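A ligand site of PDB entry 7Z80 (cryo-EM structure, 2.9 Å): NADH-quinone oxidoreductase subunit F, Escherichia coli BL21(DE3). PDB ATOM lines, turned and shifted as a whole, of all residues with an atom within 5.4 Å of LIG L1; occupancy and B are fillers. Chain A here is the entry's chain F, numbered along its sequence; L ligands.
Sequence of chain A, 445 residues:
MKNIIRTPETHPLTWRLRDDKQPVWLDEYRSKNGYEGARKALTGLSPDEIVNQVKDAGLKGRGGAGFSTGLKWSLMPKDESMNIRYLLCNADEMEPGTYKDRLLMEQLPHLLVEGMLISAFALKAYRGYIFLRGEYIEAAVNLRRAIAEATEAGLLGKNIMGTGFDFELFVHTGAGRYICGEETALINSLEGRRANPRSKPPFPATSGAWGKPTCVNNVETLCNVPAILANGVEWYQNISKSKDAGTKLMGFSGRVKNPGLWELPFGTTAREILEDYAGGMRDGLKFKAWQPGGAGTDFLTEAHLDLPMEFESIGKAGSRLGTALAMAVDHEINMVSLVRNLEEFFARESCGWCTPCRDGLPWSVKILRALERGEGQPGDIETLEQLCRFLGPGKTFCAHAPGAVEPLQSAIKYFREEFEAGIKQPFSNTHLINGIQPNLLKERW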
ATOM      1  N   GLY A  61      15.099 -18.496 -19.627  1.00  0.00           N
ATOM      2  CA  GLY A  61      14.692 -18.792 -20.991  1.00  0.00           C
ATOM      3  C   GLY A  61      15.176 -20.158 -21.427  1.00  0.00           C
ATOM      4  O   GLY A  61      16.361 -20.477 -21.322  1.00  0.00           O
ATOM      5  N   ARG A  62      14.243 -20.970 -21.913  1.00  0.00           N
ATOM      6  CA  ARG A  62      14.539 -22.342 -22.331  1.00  0.00           C
ATOM      7  C   ARG A  62      14.979 -22.434 -23.784  1.00  0.00           C
ATOM      8  O   ARG A  62      15.195 -23.537 -24.277  1.00  0.00           O
ATOM      9  CB  ARG A  62      13.331 -23.231 -22.082  1.00  0.00           C
ATOM     10  CG  ARG A  62      12.813 -23.187 -20.663  1.00  0.00           C
ATOM     11  CD  ARG A  62      13.744 -23.920 -19.723  1.00  0.00           C
ATOM     12  NE  ARG A  62      13.121 -24.238 -18.452  1.00  0.00           N
ATOM     13  CZ  ARG A  62      13.415 -23.644 -17.297  1.00  0.00           C
ATOM     14  NH1 ARG A  62      14.330 -22.688 -17.232  1.00  0.00           N
ATOM     15  NH2 ARG A  62      12.783 -24.011 -16.196  1.00  0.00           N
ATOM     16  N   GLY A  63      15.096 -21.296 -24.474  1.00  0.00           N
ATOM     17  CA  GLY A  63      15.613 -21.308 -25.830  1.00  0.00           C
ATOM     18  C   GLY A  63      17.060 -21.715 -25.931  1.00  0.00           C
ATOM     19  O   GLY A  63      17.471 -22.240 -26.968  1.00  0.00           O
ATOM     20  N   GLY A  64      17.841 -21.497 -24.874  1.00  0.00           N
ATOM     21  CA  GLY A  64      19.224 -21.905 -24.861  1.00  0.00           C
ATOM     22  C   GLY A  64      20.143 -20.899 -24.194  1.00  0.00           C
ATOM     23  O   GLY A  64      21.200 -21.272 -23.671  1.00  0.00           O
ATOM     24  N   ALA A  65      19.751 -19.629 -24.194  1.00  0.00           N
ATOM     25  CA  ALA A  65      20.589 -18.577 -23.621  1.00  0.00           C
ATOM     26  C   ALA A  65      20.409 -18.425 -22.122  1.00  0.00           C
ATOM     27  O   ALA A  65      21.302 -17.883 -21.468  1.00  0.00           O
ATOM     28  CB  ALA A  65      20.298 -17.248 -24.310  1.00  0.00           C
ATOM     29  N   GLY A  66      19.279 -18.870 -21.567  1.00  0.00           N
ATOM     30  CA  GLY A  66      19.085 -18.828 -20.138  1.00  0.00           C
ATOM     31  C   GLY A  66      18.776 -17.464 -19.557  1.00  0.00           C
ATOM     32  O   GLY A  66      19.000 -17.247 -18.366  1.00  0.00           O
ATOM     33  N   PHE A  67      18.281 -16.534 -20.367  1.00  0.00           N
ATOM     34  CA  PHE A  67      17.892 -15.228 -19.862  1.00  0.00           C
ATOM     35  C   PHE A  67      16.631 -15.337 -19.014  1.00  0.00           C
ATOM     36  O   PHE A  67      15.774 -16.199 -19.232  1.00  0.00           O
ATOM     37  CB  PHE A  67      17.653 -14.252 -21.018  1.00  0.00           C
ATOM     38  CG  PHE A  67      17.656 -12.813 -20.595  1.00  0.00           C
ATOM     39  CD1 PHE A  67      18.823 -12.190 -20.210  1.00  0.00           C
ATOM     40  CD2 PHE A  67      16.472 -12.086 -20.583  1.00  0.00           C
ATOM     41  CE1 PHE A  67      18.828 -10.863 -19.831  1.00  0.00           C
ATOM     42  CE2 PHE A  67      16.467 -10.759 -20.205  1.00  0.00           C
ATOM     43  CZ  PHE A  67      17.644 -10.149 -19.823  1.00  0.00           C
ATOM     44  N   LYS A  72      12.845 -10.129 -18.773  1.00  0.00           N
ATOM     45  CA  LYS A  72      12.510  -9.788 -20.150  1.00  0.00           C
ATOM     46  C   LYS A  72      11.104  -9.191 -20.244  1.00  0.00           C
ATOM     47  O   LYS A  72      10.876  -8.246 -21.005  1.00  0.00           O
ATOM     48  CB  LYS A  72      12.621 -11.033 -21.032  1.00  0.00           C
ATOM     49  CG  LYS A  72      12.275 -10.786 -22.487  1.00  0.00           C
ATOM     50  CD  LYS A  72      12.175 -12.085 -23.250  1.00  0.00           C
ATOM     51  CE  LYS A  72      13.446 -12.898 -23.112  1.00  0.00           C
ATOM     52  NZ  LYS A  72      13.428 -14.063 -24.034  1.00  0.00           N
ATOM     53  N   ASN A  90       8.569 -18.833 -30.337  1.00  0.00           N
ATOM     54  CA  ASN A  90       9.640 -19.277 -31.225  1.00  0.00           C
ATOM     55  C   ASN A  90       9.603 -20.798 -31.302  1.00  0.00           C
ATOM     56  O   ASN A  90      10.365 -21.516 -30.637  1.00  0.00           O
ATOM     57  CB  ASN A  90      10.982 -18.763 -30.730  1.00  0.00           C
ATOM     58  CG  ASN A  90      12.075 -18.845 -31.769  1.00  0.00           C
ATOM     59  OD1 ASN A  90      11.972 -19.575 -32.751  1.00  0.00           O
ATOM     60  ND2 ASN A  90      13.125 -18.059 -31.570  1.00  0.00           N
ATOM     61  N   ASP A  92      10.492 -22.501 -33.855  1.00  0.00           N
ATOM     62  CA  ASP A  92      11.355 -22.897 -34.963  1.00  0.00           C
ATOM     63  C   ASP A  92      12.090 -24.188 -34.642  1.00  0.00           C
ATOM     64  O   ASP A  92      11.856 -25.227 -35.268  1.00  0.00           O
ATOM     65  CB  ASP A  92      12.340 -21.780 -35.301  1.00  0.00           C
ATOM     66  CG  ASP A  92      12.625 -21.684 -36.787  1.00  0.00           C
ATOM     67  OD1 ASP A  92      11.760 -22.089 -37.589  1.00  0.00           O
ATOM     68  OD2 ASP A  92      13.718 -21.205 -37.150  1.00  0.00           O
ATOM     69  N   GLU A  93      12.961 -24.150 -33.625  1.00  0.00           N
ATOM     70  CA  GLU A  93      13.734 -25.299 -33.143  1.00  0.00           C
ATOM     71  C   GLU A  93      14.513 -25.963 -34.273  1.00  0.00           C
ATOM     72  O   GLU A  93      14.406 -27.171 -34.515  1.00  0.00           O
ATOM     73  CB  GLU A  93      12.842 -26.296 -32.419  1.00  0.00           C
ATOM     74  CG  GLU A  93      13.560 -27.118 -31.364  1.00  0.00           C
ATOM     75  CD  GLU A  93      12.872 -28.437 -31.087  1.00  0.00           C
ATOM     76  OE1 GLU A  93      12.052 -28.876 -31.920  1.00  0.00           O
ATOM     77  OE2 GLU A  93      13.153 -29.040 -30.028  1.00  0.00           O
ATOM     78  N   MET A  94      15.287 -25.152 -34.978  1.00  0.00           N
ATOM     79  CA  MET A  94      16.001 -25.587 -36.170  1.00  0.00           C
ATOM     80  C   MET A  94      17.412 -26.082 -35.867  1.00  0.00           C
ATOM     81  O   MET A  94      18.139 -26.433 -36.793  1.00  0.00           O
ATOM     82  CB  MET A  94      16.060 -24.441 -37.182  1.00  0.00           C
ATOM     83  CG  MET A  94      14.924 -24.400 -38.172  1.00  0.00           C
ATOM     84  SD  MET A  94      15.389 -24.991 -39.804  1.00  0.00           S
ATOM     85  CE  MET A  94      13.785 -25.077 -40.590  1.00  0.00           C
ATOM     86  N   GLU A  95      17.800 -26.104 -34.603  1.00  0.00           N
ATOM     87  CA  GLU A  95      19.147 -26.535 -34.217  1.00  0.00           C
ATOM     88  C   GLU A  95      19.268 -28.049 -34.317  1.00  0.00           C
ATOM     89  O   GLU A  95      18.369 -28.768 -33.876  1.00  0.00           O
ATOM     90  CB  GLU A  95      19.460 -26.082 -32.792  1.00  0.00           C
ATOM     91  CG  GLU A  95      20.834 -26.488 -32.279  1.00  0.00           C
ATOM     92  CD  GLU A  95      21.881 -25.415 -32.481  1.00  0.00           C
ATOM     93  OE1 GLU A  95      21.741 -24.606 -33.419  1.00  0.00           O
ATOM     94  OE2 GLU A  95      22.837 -25.365 -31.683  1.00  0.00           O
ATOM     95  N   ASP A 101      10.710 -29.245 -28.667  1.00  0.00           N
ATOM     96  CA  ASP A 101       9.504 -28.504 -28.997  1.00  0.00           C
ATOM     97  C   ASP A 101       8.537 -29.337 -29.831  1.00  0.00           C
ATOM     98  O   ASP A 101       7.322 -29.159 -29.730  1.00  0.00           O
ATOM     99  CB  ASP A 101       9.865 -27.214 -29.736  1.00  0.00           C
ATOM    100  CG  ASP A 101      10.757 -26.309 -28.918  1.00  0.00           C
ATOM    101  OD1 ASP A 101      10.866 -26.520 -27.694  1.00  0.00           O
ATOM    102  OD2 ASP A 101      11.360 -25.375 -29.499  1.00  0.00           O
ATOM    103  N   TYR A 178      17.223 -21.764 -41.024  1.00  0.00           N
ATOM    104  CA  TYR A 178      17.691 -21.934 -39.646  1.00  0.00           C
ATOM    105  C   TYR A 178      17.788 -20.603 -38.911  1.00  0.00           C
ATOM    106  O   TYR A 178      17.510 -20.526 -37.708  1.00  0.00           O
ATOM    107  CB  TYR A 178      19.038 -22.649 -39.649  1.00  0.00           C
ATOM    108  CG  TYR A 178      19.799 -22.595 -38.338  1.00  0.00           C
ATOM    109  CD1 TYR A 178      19.422 -23.390 -37.267  1.00  0.00           C
ATOM    110  CD2 TYR A 178      20.890 -21.766 -38.177  1.00  0.00           C
ATOM    111  CE1 TYR A 178      20.113 -23.359 -36.070  1.00  0.00           C
ATOM    112  CE2 TYR A 178      21.583 -21.726 -36.985  1.00  0.00           C
ATOM    113  CZ  TYR A 178      21.191 -22.520 -35.939  1.00  0.00           C
ATOM    114  OH  TYR A 178      21.886 -22.476 -34.761  1.00  0.00           O
ATOM    115  N   ILE A 179      18.181 -19.544 -39.627  1.00  0.00           N
ATOM    116  CA  ILE A 179      18.382 -18.229 -39.003  1.00  0.00           C
ATOM    117  C   ILE A 179      17.083 -17.593 -38.551  1.00  0.00           C
ATOM    118  O   ILE A 179      17.112 -16.657 -37.747  1.00  0.00           O
ATOM    119  CB  ILE A 179      19.147 -17.319 -39.989  1.00  0.00           C
ATOM    120  CG1 ILE A 179      19.884 -16.203 -39.250  1.00  0.00           C
ATOM    121  CG2 ILE A 179      18.209 -16.744 -41.043  1.00  0.00           C
ATOM    122  CD1 ILE A 179      20.713 -16.683 -38.083  1.00  0.00           C
ATOM    123  N   GLY A 181      15.107 -18.677 -36.423  1.00  0.00           N
ATOM    124  CA  GLY A 181      14.929 -18.874 -34.992  1.00  0.00           C
ATOM    125  C   GLY A 181      15.481 -17.751 -34.140  1.00  0.00           C
ATOM    126  O   GLY A 181      15.046 -17.588 -32.998  1.00  0.00           O
ATOM    127  N   GLU A 182      16.442 -16.987 -34.674  1.00  0.00           N
ATOM    128  CA  GLU A 182      16.908 -15.796 -33.986  1.00  0.00           C
ATOM    129  C   GLU A 182      15.762 -14.788 -33.874  1.00  0.00           C
ATOM    130  O   GLU A 182      15.028 -14.583 -34.836  1.00  0.00           O
ATOM    131  CB  GLU A 182      18.081 -15.166 -34.745  1.00  0.00           C
ATOM    132  CG  GLU A 182      19.118 -14.498 -33.858  1.00  0.00           C
ATOM    133  CD  GLU A 182      18.832 -13.033 -33.612  1.00  0.00           C
ATOM    134  OE1 GLU A 182      17.897 -12.492 -34.236  1.00  0.00           O
ATOM    135  OE2 GLU A 182      19.544 -12.417 -32.798  1.00  0.00           O
ATOM    136  N   GLU A 183      15.634 -14.183 -32.695  1.00  0.00           N
ATOM    137  CA  GLU A 183      14.403 -13.465 -32.354  1.00  0.00           C
ATOM    138  C   GLU A 183      14.169 -12.252 -33.257  1.00  0.00           C
ATOM    139  O   GLU A 183      13.031 -12.003 -33.671  1.00  0.00           O
ATOM    140  CB  GLU A 183      14.418 -13.038 -30.875  1.00  0.00           C
ATOM    141  CG  GLU A 183      15.492 -12.033 -30.523  1.00  0.00           C
ATOM    142  CD  GLU A 183      15.183 -11.268 -29.264  1.00  0.00           C
ATOM    143  OE1 GLU A 183      16.147 -10.919 -28.565  1.00  0.00           O
ATOM    144  OE2 GLU A 183      13.996 -11.037 -28.980  1.00  0.00           O
ATOM    145  N   VAL A 216       9.413 -12.208 -27.487  1.00  0.00           N
ATOM    146  CA  VAL A 216       9.642 -13.487 -28.149  1.00  0.00           C
ATOM    147  C   VAL A 216      10.125 -14.474 -27.094  1.00  0.00           C
ATOM    148  O   VAL A 216      11.101 -14.211 -26.382  1.00  0.00           O
ATOM    149  CB  VAL A 216      10.664 -13.368 -29.282  1.00  0.00           C
ATOM    150  CG1 VAL A 216      10.795 -14.686 -30.031  1.00  0.00           C
ATOM    151  CG2 VAL A 216      10.269 -12.252 -30.230  1.00  0.00           C
ATOM    152  N   ASN A 217       9.440 -15.619 -26.987  1.00  0.00           N
ATOM    153  CA  ASN A 217       9.782 -16.624 -25.992  1.00  0.00           C
ATOM    154  C   ASN A 217       9.721 -18.010 -26.624  1.00  0.00           C
ATOM    155  O   ASN A 217       8.979 -18.240 -27.576  1.00  0.00           O
ATOM    156  CB  ASN A 217       8.847 -16.560 -24.780  1.00  0.00           C
ATOM    157  CG  ASN A 217       9.303 -15.556 -23.745  1.00  0.00           C
ATOM    158  OD1 ASN A 217       8.542 -14.675 -23.353  1.00  0.00           O
ATOM    159  ND2 ASN A 217      10.545 -15.686 -23.307  1.00  0.00           N
ATOM    160  N   ASN A 218      10.503 -18.932 -26.066  1.00  0.00           N
ATOM    161  CA  ASN A 218      10.534 -20.310 -26.538  1.00  0.00           C
ATOM    162  C   ASN A 218       9.239 -21.031 -26.162  1.00  0.00           C
ATOM    163  O   ASN A 218       8.448 -20.564 -25.342  1.00  0.00           O
ATOM    164  CB  ASN A 218      11.744 -21.033 -25.966  1.00  0.00           C
ATOM    165  CG  ASN A 218      12.098 -22.297 -26.740  1.00  0.00           C
ATOM    166  OD1 ASN A 218      11.674 -22.470 -27.885  1.00  0.00           O
ATOM    167  ND2 ASN A 218      12.848 -23.181 -26.116  1.00  0.00           N
ATOM    168  N   VAL A 219       9.022 -22.184 -26.806  1.00  0.00           N
ATOM    169  CA  VAL A 219       7.873 -23.036 -26.486  1.00  0.00           C
ATOM    170  C   VAL A 219       7.953 -23.535 -25.058  1.00  0.00           C
ATOM    171  O   VAL A 219       6.958 -23.545 -24.331  1.00  0.00           O
ATOM    172  CB  VAL A 219       7.788 -24.206 -27.485  1.00  0.00           C
ATOM    173  CG1 VAL A 219       6.509 -24.982 -27.261  1.00  0.00           C
ATOM    174  CG2 VAL A 219       7.867 -23.711 -28.895  1.00  0.00           C
ATOM    175  N   THR A 221       9.486 -22.344 -22.409  1.00  0.00           N
ATOM    176  CA  THR A 221       9.245 -21.310 -21.404  1.00  0.00           C
ATOM    177  C   THR A 221       7.747 -21.083 -21.206  1.00  0.00           C
ATOM    178  O   THR A 221       7.257 -21.015 -20.069  1.00  0.00           O
ATOM    179  CB  THR A 221       9.931 -20.018 -21.828  1.00  0.00           C
ATOM    180  OG1 THR A 221      11.310 -20.279 -22.109  1.00  0.00           O
ATOM    181  CG2 THR A 221       9.825 -18.984 -20.732  1.00  0.00           C
ATOM    182  N   CYS A 398      25.337 -11.255 -35.485  1.00  0.00           N
ATOM    183  CA  CYS A 398      24.505 -12.040 -34.587  1.00  0.00           C
ATOM    184  C   CYS A 398      25.298 -13.199 -34.006  1.00  0.00           C
ATOM    185  O   CYS A 398      26.510 -13.283 -34.214  1.00  0.00           O
ATOM    186  CB  CYS A 398      23.240 -12.532 -35.308  1.00  0.00           C
ATOM    187  SG  CYS A 398      23.399 -14.125 -36.125  1.00  0.00           S
ATOM    188  N   ALA A 399      24.627 -14.098 -33.284  1.00  0.00           N
ATOM    189  CA  ALA A 399      25.303 -15.160 -32.546  1.00  0.00           C
ATOM    190  C   ALA A 399      25.285 -16.500 -33.274  1.00  0.00           C
ATOM    191  O   ALA A 399      25.537 -17.531 -32.657  1.00  0.00           O
ATOM    192  CB  ALA A 399      24.686 -15.303 -31.148  1.00  0.00           C
ATOM    193  N   HIS A 400      24.965 -16.495 -34.574  1.00  0.00           N
ATOM    194  CA  HIS A 400      25.013 -17.732 -35.345  1.00  0.00           C
ATOM    195  C   HIS A 400      26.445 -18.233 -35.503  1.00  0.00           C
ATOM    196  O   HIS A 400      26.704 -19.431 -35.380  1.00  0.00           O
ATOM    197  CB  HIS A 400      24.364 -17.497 -36.720  1.00  0.00           C
ATOM    198  CG  HIS A 400      24.678 -18.549 -37.737  1.00  0.00           C
ATOM    199  ND1 HIS A 400      23.922 -19.694 -37.881  1.00  0.00           N
ATOM    200  CD2 HIS A 400      25.640 -18.619 -38.679  1.00  0.00           C
ATOM    201  CE1 HIS A 400      24.420 -20.425 -38.852  1.00  0.00           C
ATOM    202  NE2 HIS A 400      25.460 -19.796 -39.360  1.00  0.00           N
HETATM  203  N1  LIG L   1      15.385 -19.768 -29.962  1.00  0.00           N
HETATM  204  C1  LIG L   1      14.320 -20.630 -30.113  1.00  0.00           C
HETATM  205  O1  LIG L   1      13.472 -20.706 -29.223  1.00  0.00           O
HETATM  206  N2  LIG L   1      14.196 -21.390 -31.254  1.00  0.00           N
HETATM  207  C2  LIG L   1      15.157 -21.290 -32.239  1.00  0.00           C
HETATM  208  O2  LIG L   1      15.064 -21.972 -33.256  1.00  0.00           O
HETATM  209  C3  LIG L   1      16.222 -20.428 -32.088  1.00  0.00           C
HETATM  210  N3  LIG L   1      17.181 -20.336 -33.070  1.00  0.00           N
HETATM  211  C4  LIG L   1      18.236 -19.474 -32.920  1.00  0.00           C
HETATM  212  C5  LIG L   1      19.180 -19.395 -33.932  1.00  0.00           C
HETATM  213  C6  LIG L   1      20.258 -18.543 -33.796  1.00  0.00           C
HETATM  214  C7  LIG L   1      21.270 -18.472 -34.895  1.00  0.00           C
HETATM  215  C8  LIG L   1      20.393 -17.760 -32.654  1.00  0.00           C
HETATM  216  C9  LIG L   1      21.564 -16.838 -32.505  1.00  0.00           C
HETATM  217  C10 LIG L   1      19.448 -17.839 -31.642  1.00  0.00           C
HETATM  218  C11 LIG L   1      18.360 -18.700 -31.775  1.00  0.00           C
HETATM  219  N4  LIG L   1      17.397 -18.796 -30.781  1.00  0.00           N
HETATM  220  C12 LIG L   1      16.334 -19.662 -30.941  1.00  0.00           C
HETATM  221  C13 LIG L   1      17.479 -17.979 -29.517  1.00  0.00           C
HETATM  222  C14 LIG L   1      16.704 -16.672 -29.682  1.00  0.00           C
HETATM  223  O3  LIG L   1      17.589 -15.634 -30.007  1.00  0.00           O
HETATM  224  C15 LIG L   1      15.932 -16.295 -28.423  1.00  0.00           C
HETATM  225  O4  LIG L   1      16.638 -16.740 -27.294  1.00  0.00           O
HETATM  226  C16 LIG L   1      14.535 -16.904 -28.421  1.00  0.00           C
HETATM  227  O5  LIG L   1      13.782 -16.339 -29.483  1.00  0.00           O
HETATM  228  C17 LIG L   1      13.814 -16.664 -27.104  1.00  0.00           C
HETATM  229  O6  LIG L   1      14.629 -17.125 -26.063  1.00  0.00           O
HETATM  230  P1  LIG L   1      14.042 -17.306 -24.573  1.00  0.00           P
HETATM  231  O7  LIG L   1      13.668 -18.748 -24.372  1.00  0.00           O
HETATM  232  O8  LIG L   1      15.116 -16.900 -23.588  1.00  0.00           O
HETATM  233  O9  LIG L   1      12.821 -16.442 -24.387  1.00  0.00           O
HETATM  234  P1  LG2 L   2      21.142 -13.316 -26.339  1.00  0.00           P
HETATM  235  O1  LG2 L   2      21.719 -13.963 -25.138  1.00  0.00           O
HETATM  236  O2  LG2 L   2      21.651 -11.909 -26.613  1.00  0.00           O
HETATM  237  O3  LG2 L   2      19.550 -13.213 -26.217  1.00  0.00           O
HETATM  238  C1  LG2 L   2      18.722 -14.263 -25.671  1.00  0.00           C
HETATM  239  C2  LG2 L   2      17.512 -13.649 -25.010  1.00  0.00           C
HETATM  240  O4  LG2 L   2      17.933 -12.782 -23.943  1.00  0.00           O
HETATM  241  C3  LG2 L   2      16.627 -12.808 -25.942  1.00  0.00           C
HETATM  242  O5  LG2 L   2      15.247 -13.126 -25.781  1.00  0.00           O
HETATM  243  C4  LG2 L   2      16.960 -11.371 -25.531  1.00  0.00           C
HETATM  244  O6  LG2 L   2      15.830 -10.504 -25.696  1.00  0.00           O
HETATM  245  C5  LG2 L   2      17.299 -11.520 -24.060  1.00  0.00           C
HETATM  246  N1  LG2 L   2      18.222 -10.510 -23.566  1.00  0.00           N
HETATM  247  C6  LG2 L   2      19.564 -10.650 -23.322  1.00  0.00           C
HETATM  248  N2  LG2 L   2      20.141  -9.569 -22.866  1.00  0.00           N
HETATM  249  C7  LG2 L   2      19.107  -8.636 -22.822  1.00  0.00           C
HETATM  250  C8  LG2 L   2      19.058  -7.293 -22.426  1.00  0.00           C
HETATM  251  N3  LG2 L   2      20.114  -6.609 -21.978  1.00  0.00           N
HETATM  252  N4  LG2 L   2      17.867  -6.655 -22.505  1.00  0.00           N
HETATM  253  C9  LG2 L   2      16.813  -7.330 -22.958  1.00  0.00           C
HETATM  254  N5  LG2 L   2      16.731  -8.602 -23.344  1.00  0.00           N
HETATM  255  C10 LG2 L   2      17.922  -9.214 -23.256  1.00  0.00           C
HETATM  256  O7  LG2 L   2      21.425 -14.169 -27.648  1.00  0.00           O
HETATM  257  P2  LG2 L   2      20.561 -14.731 -28.858  1.00  0.00           P
HETATM  258  O8  LG2 L   2      21.382 -14.515 -30.134  1.00  0.00           O
HETATM  259  O9  LG2 L   2      19.194 -14.185 -28.907  1.00  0.00           O
HETATM  260  O10 LG2 L   2      20.554 -16.316 -28.600  1.00  0.00           O
HETATM  261  C11 LG2 L   2      21.785 -17.078 -28.598  1.00  0.00           C
HETATM  262  C12 LG2 L   2      21.541 -18.419 -27.949  1.00  0.00           C
HETATM  263  O11 LG2 L   2      20.472 -19.094 -28.632  1.00  0.00           O
HETATM  264  C13 LG2 L   2      22.715 -19.384 -28.033  1.00  0.00           C
HETATM  265  O12 LG2 L   2      23.628 -19.160 -26.968  1.00  0.00           O
HETATM  266  C14 LG2 L   2      22.040 -20.753 -27.944  1.00  0.00           C
HETATM  267  O13 LG2 L   2      22.067 -21.268 -26.608  1.00  0.00           O
HETATM  268  C15 LG2 L   2      20.595 -20.486 -28.397  1.00  0.00           C
HETATM  269  N6  LG2 L   2      20.227 -21.195 -29.628  1.00  0.00           N
HETATM  270  C16 LG2 L   2      19.066 -21.971 -29.681  1.00  0.00           C
HETATM  271  C17 LG2 L   2      18.683 -22.643 -30.775  1.00  0.00           C
HETATM  272  C18 LG2 L   2      17.442 -23.440 -30.693  1.00  0.00           C
HETATM  273  O14 LG2 L   2      16.875 -23.610 -29.604  1.00  0.00           O
HETATM  274  N7  LG2 L   2      16.971 -23.978 -31.815  1.00  0.00           N
HETATM  275  C19 LG2 L   2      19.493 -22.565 -32.037  1.00  0.00           C
HETATM  276  C20 LG2 L   2      20.715 -21.740 -31.863  1.00  0.00           C
HETATM  277  C21 LG2 L   2      21.015 -21.125 -30.730  1.00  0.00           C
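An oxygen (O9) of LIG L1 is in salt-bridge range of the side-chain amino group of Lys 72 (2.5 Å).
The side-chain amide nitrogen (ND2) of Asn 217 is in hydrogen-bond range of an oxygen (O9) of LIG L1.
O5 of LIG L1 sits at hydrogen-bond distance from ND2 of Asn 90 (2.8 Å).
An oxygen (O1) of LIG L1 sits close to the side-chain amide oxygen (OD1) of Asn 218 (2.9 Å).
The backbone NH (N) of Gly 63 is in hydrogen-bond range of an oxygen (O7) of LIG L1, 2.9 Å away.
An oxygen (O2) of LIG L1 lies within hydrogen-bond range of the backbone NH of Glu 93, 3.0 Å away.
N of Arg 62 lies within hydrogen-bond range of O7 of LIG L1 (3.4 Å).
The side-chain amino group (NZ) of Lys 72 is in hydrogen-bond range of an oxygen (O5) of LG2 L2, at 2.7 Å.
OE1 of Glu 183 is in hydrogen-bond range of O6 of LG2 L2, at 2.9 Å.
The backbone carbonyl oxygen (O) of Gly 64 is in hydrogen-bond range of an oxygen (O13) of LG2 L2 (3.1 Å).
An oxygen (O3) of LIG L1 sits at hydrogen-bond distance from an oxygen (O9) of LG2 L2, 2.4 Å away.
NZ of Lys 72 lies close to ND2 of Asn 217 (3.4 Å).
The backbone carbonyl oxygen (O) of Asn 217 sits at hydrogen-bond distance from the backbone NH (N) of Asn 90, at 2.9 Å.
The side-chain amide oxygen (OD1) of Asn 218 sits close to the backbone carbonyl oxygen (O) of Asn 90, 3.2 Å away.
N of Gly 63 lies close to ND2 of Asn 218, at 3.4 Å.
The side-chain amide nitrogen of Asn 218 sits at hydrogen-bond distance from the backbone carbonyl oxygen of Arg 62 (3.0 Å).
The side-chain carboxylate (OE2) of Glu 93 is in hydrogen-bond range of the backbone NH (N) of Asp 101, 2.8 Å away.
N of His 400 lies close to SG of Cys 398 (3.2 Å).
The side-chain carboxylate (OE1) of Glu 95 is in hydrogen-bond range of the side-chain hydroxyl (OH) of Tyr 178 (2.5 Å).
N4 of LIG L1 lies close to O of Gly 181 (3.4 Å).
The backbone carbonyl oxygen (O) of Val 216 sits close to an oxygen (O9) of LIG L1, at 3.5 Å.
Merely in contact with LIG L1: Gly 61 (3.2 Å), Asp 92 (3.4 Å), Glu 182 (3.5 Å), Thr 221 (3.6 Å), Met 94 (3.6 Å), Glu 183 (3.6 Å), Ile 179 (3.7 Å), His 400 (3.7 Å), Ala 399 (3.7 Å) and Tyr 178 (3.9 Å).
Hydrophobic or aromatic side chains within 4 Å of LIG L1: Tyr 178, Ile 179, Val 216, Ala 399 and His 400.
The nearest printed residue that does not touch LIG L1 is Phe 67 (4.5 Å).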
